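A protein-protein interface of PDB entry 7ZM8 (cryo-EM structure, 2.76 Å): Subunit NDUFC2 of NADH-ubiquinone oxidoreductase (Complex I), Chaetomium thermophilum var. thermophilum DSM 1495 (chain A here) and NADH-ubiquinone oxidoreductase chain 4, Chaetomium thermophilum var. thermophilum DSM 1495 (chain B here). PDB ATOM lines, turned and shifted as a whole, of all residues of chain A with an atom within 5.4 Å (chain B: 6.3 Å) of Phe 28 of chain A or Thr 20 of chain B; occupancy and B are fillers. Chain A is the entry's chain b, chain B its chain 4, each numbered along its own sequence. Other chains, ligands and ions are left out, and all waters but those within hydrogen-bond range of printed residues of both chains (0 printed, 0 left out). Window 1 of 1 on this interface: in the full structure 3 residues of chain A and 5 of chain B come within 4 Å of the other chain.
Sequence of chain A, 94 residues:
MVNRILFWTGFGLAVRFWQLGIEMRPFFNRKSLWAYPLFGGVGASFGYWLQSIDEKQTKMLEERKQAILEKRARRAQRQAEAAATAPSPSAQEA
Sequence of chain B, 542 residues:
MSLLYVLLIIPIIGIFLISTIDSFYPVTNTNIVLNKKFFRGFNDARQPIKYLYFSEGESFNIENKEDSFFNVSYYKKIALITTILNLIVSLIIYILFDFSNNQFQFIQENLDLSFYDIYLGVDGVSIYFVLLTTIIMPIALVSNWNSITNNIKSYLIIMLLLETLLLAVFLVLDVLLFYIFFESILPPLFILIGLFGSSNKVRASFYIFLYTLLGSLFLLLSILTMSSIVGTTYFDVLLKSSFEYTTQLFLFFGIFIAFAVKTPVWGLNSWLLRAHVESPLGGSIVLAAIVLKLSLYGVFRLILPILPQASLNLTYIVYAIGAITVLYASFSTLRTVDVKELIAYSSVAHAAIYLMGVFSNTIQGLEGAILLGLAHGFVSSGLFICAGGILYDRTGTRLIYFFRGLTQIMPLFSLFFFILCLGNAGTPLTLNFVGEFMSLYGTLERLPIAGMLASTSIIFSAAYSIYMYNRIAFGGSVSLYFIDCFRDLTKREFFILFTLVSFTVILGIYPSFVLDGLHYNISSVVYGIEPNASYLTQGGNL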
ATOM      1  N   PHE A  17     -20.456 -20.124 -31.072  1.00  0.00           N
ATOM      2  CA  PHE A  17     -19.257 -19.355 -30.759  1.00  0.00           C
ATOM      3  C   PHE A  17     -18.004 -20.048 -31.263  1.00  0.00           C
ATOM      4  O   PHE A  17     -17.106 -19.401 -31.812  1.00  0.00           O
ATOM      5  CB  PHE A  17     -19.161 -19.130 -29.255  1.00  0.00           C
ATOM      6  CG  PHE A  17     -19.867 -17.905 -28.789  1.00  0.00           C
ATOM      7  CD1 PHE A  17     -19.415 -16.654 -29.155  1.00  0.00           C
ATOM      8  CD2 PHE A  17     -20.992 -18.001 -27.990  1.00  0.00           C
ATOM      9  CE1 PHE A  17     -20.068 -15.532 -28.729  1.00  0.00           C
ATOM     10  CE2 PHE A  17     -21.651 -16.877 -27.563  1.00  0.00           C
ATOM     11  CZ  PHE A  17     -21.192 -15.643 -27.932  1.00  0.00           C
ATOM     12  N   LEU A  20     -17.656 -19.916 -35.302  1.00  0.00           N
ATOM     13  CA  LEU A  20     -17.126 -18.684 -35.864  1.00  0.00           C
ATOM     14  C   LEU A  20     -15.664 -18.495 -35.502  1.00  0.00           C
ATOM     15  O   LEU A  20     -14.904 -17.927 -36.289  1.00  0.00           O
ATOM     16  CB  LEU A  20     -17.972 -17.501 -35.398  1.00  0.00           C
ATOM     17  CG  LEU A  20     -19.475 -17.653 -35.665  1.00  0.00           C
ATOM     18  CD1 LEU A  20     -20.266 -16.469 -35.152  1.00  0.00           C
ATOM     19  CD2 LEU A  20     -19.734 -17.870 -37.134  1.00  0.00           C
ATOM     20  N   PRO A  26     -16.261 -12.805 -37.674  1.00  0.00           N
ATOM     21  CA  PRO A  26     -16.529 -11.924 -36.538  1.00  0.00           C
ATOM     22  C   PRO A  26     -17.689 -12.382 -35.646  1.00  0.00           C
ATOM     23  O   PRO A  26     -18.784 -12.502 -36.132  1.00  0.00           O
ATOM     24  CB  PRO A  26     -16.944 -10.588 -37.168  1.00  0.00           C
ATOM     25  CG  PRO A  26     -17.501 -10.957 -38.520  1.00  0.00           C
ATOM     26  CD  PRO A  26     -16.705 -12.172 -38.938  1.00  0.00           C
ATOM     27  N   PHE A  27     -17.429 -12.643 -34.368  1.00  0.00           N
ATOM     28  CA  PHE A  27     -18.566 -12.957 -33.471  1.00  0.00           C
ATOM     29  C   PHE A  27     -19.406 -11.688 -33.369  1.00  0.00           C
ATOM     30  O   PHE A  27     -18.788 -10.607 -33.320  1.00  0.00           O
ATOM     31  CB  PHE A  27     -18.087 -13.243 -32.048  1.00  0.00           C
ATOM     32  CG  PHE A  27     -16.960 -14.225 -31.874  1.00  0.00           C
ATOM     33  CD1 PHE A  27     -17.099 -15.548 -32.257  1.00  0.00           C
ATOM     34  CD2 PHE A  27     -15.776 -13.836 -31.270  1.00  0.00           C
ATOM     35  CE1 PHE A  27     -16.061 -16.446 -32.073  1.00  0.00           C
ATOM     36  CE2 PHE A  27     -14.740 -14.736 -31.086  1.00  0.00           C
ATOM     37  CZ  PHE A  27     -14.885 -16.043 -31.487  1.00  0.00           C
ATOM     38  N   PHE A  28     -20.730 -11.782 -33.442  1.00  0.00           N
ATOM     39  CA  PHE A  28     -21.618 -10.607 -33.185  1.00  0.00           C
ATOM     40  C   PHE A  28     -21.869  -9.686 -34.377  1.00  0.00           C
ATOM     41  O   PHE A  28     -22.077  -8.492 -34.132  1.00  0.00           O
ATOM     42  CB  PHE A  28     -21.276  -9.849 -31.899  1.00  0.00           C
ATOM     43  CG  PHE A  28     -21.138 -10.718 -30.678  1.00  0.00           C
ATOM     44  CD1 PHE A  28     -22.161 -11.567 -30.294  1.00  0.00           C
ATOM     45  CD2 PHE A  28     -19.984 -10.686 -29.915  1.00  0.00           C
ATOM     46  CE1 PHE A  28     -22.030 -12.367 -29.173  1.00  0.00           C
ATOM     47  CE2 PHE A  28     -19.853 -11.487 -28.793  1.00  0.00           C
ATOM     48  CZ  PHE A  28     -20.879 -12.319 -28.421  1.00  0.00           C
ATOM     49  N   ASN A  29     -21.869 -10.196 -35.609  1.00  0.00           N
ATOM     50  CA  ASN A  29     -22.313  -9.352 -36.749  1.00  0.00           C
ATOM     51  C   ASN A  29     -23.833  -9.253 -36.588  1.00  0.00           C
ATOM     52  O   ASN A  29     -24.457 -10.309 -36.396  1.00  0.00           O
ATOM     53  CB  ASN A  29     -21.866  -9.926 -38.096  1.00  0.00           C
ATOM     54  CG  ASN A  29     -22.790  -9.587 -39.248  1.00  0.00           C
ATOM     55  OD1 ASN A  29     -23.155  -8.431 -39.451  1.00  0.00           O
ATOM     56  ND2 ASN A  29     -23.158 -10.590 -40.024  1.00  0.00           N
ATOM     57  N   ARG A  30     -24.408  -8.057 -36.688  1.00  0.00           N
ATOM     58  CA  ARG A  30     -25.859  -7.868 -36.420  1.00  0.00           C
ATOM     59  C   ARG A  30     -26.742  -8.637 -37.408  1.00  0.00           C
ATOM     60  O   ARG A  30     -27.723  -9.236 -36.949  1.00  0.00           O
ATOM     61  CB  ARG A  30     -26.212  -6.379 -36.431  1.00  0.00           C
ATOM     62  CG  ARG A  30     -25.989  -5.667 -35.103  1.00  0.00           C
ATOM     63  CD  ARG A  30     -24.528  -5.479 -34.738  1.00  0.00           C
ATOM     64  NE  ARG A  30     -24.335  -4.996 -33.378  1.00  0.00           N
ATOM     65  CZ  ARG A  30     -24.183  -5.777 -32.315  1.00  0.00           C
ATOM     66  NH1 ARG A  30     -24.206  -7.092 -32.449  1.00  0.00           N
ATOM     67  NH2 ARG A  30     -24.014  -5.242 -31.120  1.00  0.00           N
ATOM     68  N   LEU A  33     -27.062 -12.248 -36.264  1.00  0.00           N
ATOM     69  CA  LEU A  33     -27.271 -12.557 -34.855  1.00  0.00           C
ATOM     70  C   LEU A  33     -28.336 -13.619 -34.643  1.00  0.00           C
ATOM     71  O   LEU A  33     -28.334 -14.279 -33.601  1.00  0.00           O
ATOM     72  CB  LEU A  33     -27.658 -11.297 -34.088  1.00  0.00           C
ATOM     73  CG  LEU A  33     -26.505 -10.395 -33.676  1.00  0.00           C
ATOM     74  CD1 LEU A  33     -27.035  -9.160 -32.989  1.00  0.00           C
ATOM     75  CD2 LEU A  33     -25.520 -11.138 -32.797  1.00  0.00           C
ATOM     76  N   TYR A  36     -27.650 -17.247 -33.180  1.00  0.00           N
ATOM     77  CA  TYR A  36     -27.574 -17.571 -31.758  1.00  0.00           C
ATOM     78  C   TYR A  36     -28.901 -18.069 -31.196  1.00  0.00           C
ATOM     79  O   TYR A  36     -28.898 -19.096 -30.499  1.00  0.00           O
ATOM     80  CB  TYR A  36     -27.038 -16.364 -30.981  1.00  0.00           C
ATOM     81  CG  TYR A  36     -25.570 -16.123 -31.189  1.00  0.00           C
ATOM     82  CD1 TYR A  36     -24.628 -17.001 -30.688  1.00  0.00           C
ATOM     83  CD2 TYR A  36     -25.123 -15.021 -31.893  1.00  0.00           C
ATOM     84  CE1 TYR A  36     -23.288 -16.785 -30.873  1.00  0.00           C
ATOM     85  CE2 TYR A  36     -23.784 -14.799 -32.086  1.00  0.00           C
ATOM     86  CZ  TYR A  36     -22.869 -15.683 -31.573  1.00  0.00           C
ATOM     87  OH  TYR A  36     -21.527 -15.463 -31.768  1.00  0.00           O
ATOM     88  N   ILE B  15     -12.541 -15.184 -18.925  1.00  0.00           N
ATOM     89  CA  ILE B  15     -12.077 -15.775 -20.175  1.00  0.00           C
ATOM     90  C   ILE B  15     -12.980 -15.353 -21.324  1.00  0.00           C
ATOM     91  O   ILE B  15     -12.504 -15.013 -22.413  1.00  0.00           O
ATOM     92  CB  ILE B  15     -12.008 -17.307 -20.050  1.00  0.00           C
ATOM     93  CG1 ILE B  15     -10.860 -17.726 -19.133  1.00  0.00           C
ATOM     94  CG2 ILE B  15     -11.851 -17.948 -21.421  1.00  0.00           C
ATOM     95  CD1 ILE B  15     -10.669 -19.217 -19.048  1.00  0.00           C
ATOM     96  N   PHE B  16     -14.295 -15.364 -21.099  1.00  0.00           N
ATOM     97  CA  PHE B  16     -15.233 -14.979 -22.149  1.00  0.00           C
ATOM     98  C   PHE B  16     -15.055 -13.524 -22.559  1.00  0.00           C
ATOM     99  O   PHE B  16     -15.084 -13.198 -23.749  1.00  0.00           O
ATOM    100  CB  PHE B  16     -16.667 -15.221 -21.688  1.00  0.00           C
ATOM    101  CG  PHE B  16     -17.691 -14.885 -22.726  1.00  0.00           C
ATOM    102  CD1 PHE B  16     -17.906 -15.732 -23.802  1.00  0.00           C
ATOM    103  CD2 PHE B  16     -18.432 -13.723 -22.638  1.00  0.00           C
ATOM    104  CE1 PHE B  16     -18.844 -15.426 -24.766  1.00  0.00           C
ATOM    105  CE2 PHE B  16     -19.369 -13.417 -23.593  1.00  0.00           C
ATOM    106  CZ  PHE B  16     -19.576 -14.270 -24.659  1.00  0.00           C
ATOM    107  N   LEU B  17     -14.829 -12.641 -21.599  1.00  0.00           N
ATOM    108  CA  LEU B  17     -14.761 -11.198 -21.927  1.00  0.00           C
ATOM    109  C   LEU B  17     -13.490 -10.866 -22.709  1.00  0.00           C
ATOM    110  O   LEU B  17     -13.578 -10.069 -23.636  1.00  0.00           O
ATOM    111  CB  LEU B  17     -14.900 -10.399 -20.631  1.00  0.00           C
ATOM    112  CG  LEU B  17     -16.250 -10.533 -19.933  1.00  0.00           C
ATOM    113  CD1 LEU B  17     -16.229  -9.848 -18.578  1.00  0.00           C
ATOM    114  CD2 LEU B  17     -17.360  -9.972 -20.803  1.00  0.00           C
ATOM    115  N   ILE B  18     -12.369 -11.489 -22.373  1.00  0.00           N
ATOM    116  CA  ILE B  18     -11.096 -11.279 -23.111  1.00  0.00           C
ATOM    117  C   ILE B  18     -11.308 -11.740 -24.550  1.00  0.00           C
ATOM    118  O   ILE B  18     -10.881 -11.038 -25.467  1.00  0.00           O
ATOM    119  CB  ILE B  18      -9.980 -12.066 -22.398  1.00  0.00           C
ATOM    120  CG1 ILE B  18      -9.691 -11.486 -21.013  1.00  0.00           C
ATOM    121  CG2 ILE B  18      -8.721 -12.143 -23.243  1.00  0.00           C
ATOM    122  CD1 ILE B  18      -8.783 -12.345 -20.175  1.00  0.00           C
ATOM    123  N   SER B  19     -11.986 -12.858 -24.732  1.00  0.00           N
ATOM    124  CA  SER B  19     -12.254 -13.437 -26.067  1.00  0.00           C
ATOM    125  C   SER B  19     -13.214 -12.590 -26.906  1.00  0.00           C
ATOM    126  O   SER B  19     -13.128 -12.687 -28.137  1.00  0.00           O
ATOM    127  CB  SER B  19     -12.729 -14.840 -25.906  1.00  0.00           C
ATOM    128  OG  SER B  19     -11.899 -15.546 -25.000  1.00  0.00           O
ATOM    129  N   THR B  20     -14.131 -11.844 -26.291  1.00  0.00           N
ATOM    130  CA  THR B  20     -15.154 -11.088 -27.065  1.00  0.00           C
ATOM    131  C   THR B  20     -14.921  -9.568 -27.164  1.00  0.00           C
ATOM    132  O   THR B  20     -15.656  -8.957 -27.916  1.00  0.00           O
ATOM    133  CB  THR B  20     -16.557 -11.404 -26.536  1.00  0.00           C
ATOM    134  OG1 THR B  20     -16.581 -11.130 -25.135  1.00  0.00           O
ATOM    135  CG2 THR B  20     -16.958 -12.841 -26.781  1.00  0.00           C
ATOM    136  N   ILE B  21     -13.973  -8.965 -26.447  1.00  0.00           N
ATOM    137  CA  ILE B  21     -13.838  -7.467 -26.452  1.00  0.00           C
ATOM    138  C   ILE B  21     -13.398  -6.921 -27.814  1.00  0.00           C
ATOM    139  O   ILE B  21     -13.873  -5.844 -28.179  1.00  0.00           O
ATOM    140  CB  ILE B  21     -13.036  -6.892 -25.265  1.00  0.00           C
ATOM    141  CG1 ILE B  21     -11.664  -7.537 -25.085  1.00  0.00           C
ATOM    142  CG2 ILE B  21     -13.859  -6.924 -23.988  1.00  0.00           C
ATOM    143  CD1 ILE B  21     -10.662  -6.598 -24.466  1.00  0.00           C
ATOM    144  N   ASP B  22     -12.488  -7.700 -28.507  1.00  0.00           N
ATOM    145  CA  ASP B  22     -12.035  -7.340 -29.876  1.00  0.00           C
ATOM    146  C   ASP B  22     -13.247  -7.238 -30.807  1.00  0.00           C
ATOM    147  O   ASP B  22     -13.157  -6.506 -31.800  1.00  0.00           O
ATOM    148  CB  ASP B  22     -10.995  -8.353 -30.352  1.00  0.00           C
ATOM    149  CG  ASP B  22     -10.638  -8.297 -31.828  1.00  0.00           C
ATOM    150  OD1 ASP B  22      -9.584  -7.719 -32.149  1.00  0.00           O
ATOM    151  OD2 ASP B  22     -11.393  -8.868 -32.642  1.00  0.00           O
ATOM    152  N   SER B  23     -14.349  -7.863 -30.480  1.00  0.00           N
ATOM    153  CA  SER B  23     -15.567  -7.878 -31.328  1.00  0.00           C
ATOM    154  C   SER B  23     -16.421  -6.637 -31.064  1.00  0.00           C
ATOM    155  O   SER B  23     -17.519  -6.558 -31.620  1.00  0.00           O
ATOM    156  CB  SER B  23     -16.351  -9.132 -31.132  1.00  0.00           C
ATOM    157  OG  SER B  23     -17.340  -8.946 -30.138  1.00  0.00           O
ATOM    158  N   PHE B  24     -15.931  -5.705 -30.254  1.00  0.00           N
ATOM    159  CA  PHE B  24     -16.653  -4.471 -30.006  1.00  0.00           C
ATOM    160  C   PHE B  24     -15.823  -3.224 -30.257  1.00  0.00           C
ATOM    161  O   PHE B  24     -16.293  -2.122 -29.955  1.00  0.00           O
ATOM    162  CB  PHE B  24     -17.175  -4.445 -28.563  1.00  0.00           C
ATOM    163  CG  PHE B  24     -18.043  -5.614 -28.220  1.00  0.00           C
ATOM    164  CD1 PHE B  24     -19.260  -5.796 -28.848  1.00  0.00           C
ATOM    165  CD2 PHE B  24     -17.627  -6.552 -27.294  1.00  0.00           C
ATOM    166  CE1 PHE B  24     -20.055  -6.876 -28.542  1.00  0.00           C
ATOM    167  CE2 PHE B  24     -18.416  -7.636 -26.983  1.00  0.00           C
ATOM    168  CZ  PHE B  24     -19.632  -7.800 -27.607  1.00  0.00           C
ATOM    169  N   LYS B 153      -3.281 -12.463 -24.878  1.00  0.00           N
ATOM    170  CA  LYS B 153      -4.623 -13.036 -24.614  1.00  0.00           C
ATOM    171  C   LYS B 153      -4.512 -14.496 -24.217  1.00  0.00           C
ATOM    172  O   LYS B 153      -5.120 -14.885 -23.231  1.00  0.00           O
ATOM    173  CB  LYS B 153      -5.454 -13.032 -25.891  1.00  0.00           C
ATOM    174  CG  LYS B 153      -6.052 -11.694 -26.293  1.00  0.00           C
ATOM    175  CD  LYS B 153      -7.011 -11.808 -27.448  1.00  0.00           C
ATOM    176  CE  LYS B 153      -8.173 -12.728 -27.159  1.00  0.00           C
ATOM    177  NZ  LYS B 153      -9.084 -12.828 -28.321  1.00  0.00           N
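The backbone carbonyl oxygen (O) of Thr 20 of chain B is in hydrogen-bond range of the side-chain hydroxyl (OG) of Ser 23 of chain B, 2.8 Å away.
O of Phe 28 of chain A sits at hydrogen-bond distance from NH1 of Arg 30 of chain A.
The side-chain hydroxyl (OG1) of Thr 20 of chain B lies within hydrogen-bond range of the backbone carbonyl oxygen (O) of Phe 16 of chain B, 2.9 Å away.
The backbone carbonyl oxygen (O) of Ile 15 of chain B is in hydrogen-bond range of the side-chain hydroxyl (OG) of Ser 19 of chain B, 2.7 Å away.
Of chain B, only Thr 20 (3.8 Å), Ser 23 (3.2 Å) and Phe 24 (3.7 Å) come within 4 Å of Phe 28 of chain A.
Thr 20 of chain B touches just one residue of chain A: Phe 28.
Of the printed residues of chain A, Ser 19 of chain B touches Phe 27 (3.9 Å).
Printed residues of chain A within 4 Å of Ser 23 of chain B: Phe 27 and Phe 28.
Of the printed residues of chain A, Phe 16 of chain B touches Phe 17.
Printed residues of chain A within 4 Å of Phe 24 of chain B: Phe 28.
Arg 30 of chain A touches none of the printed residues of chain B.
Asn 29 of chain A touches none of the printed residues of chain B.
The nearest residue of chain A that does not touch Thr 20 of chain B is Phe 17 of chain A (4.6 Å).
Of the 9 printed residues of chain A, 3 touch a printed residue of chain B.
Along chain A the printed residues that touch a printed residue of chain B span positions 17 to 28.
Hydrophobic or aromatic side chains of chain B that line the printed part of chain A: Phe 16 and Phe 24.
Among the printed residues, no Asp or Glu carboxylate lies within 4 Å of a Lys or Arg side-chain nitrogen of the other chain.
Among the printed residues, merely in contact across the chains: Phe 28 of chain A with Ser 23 of chain B (3.2 Å), Phe 27 of chain A with Ser 23 of chain B (3.6 Å), Phe 28 of chain A with Phe 24 of chain B (3.7 Å), Phe 28 of chain A with Thr 20 of chain B (3.8 Å), Phe 17 of chain A with Phe 16 of chain B (3.9 Å) and Phe 27 of chain A with Ser 19 of chain B (3.9 Å).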
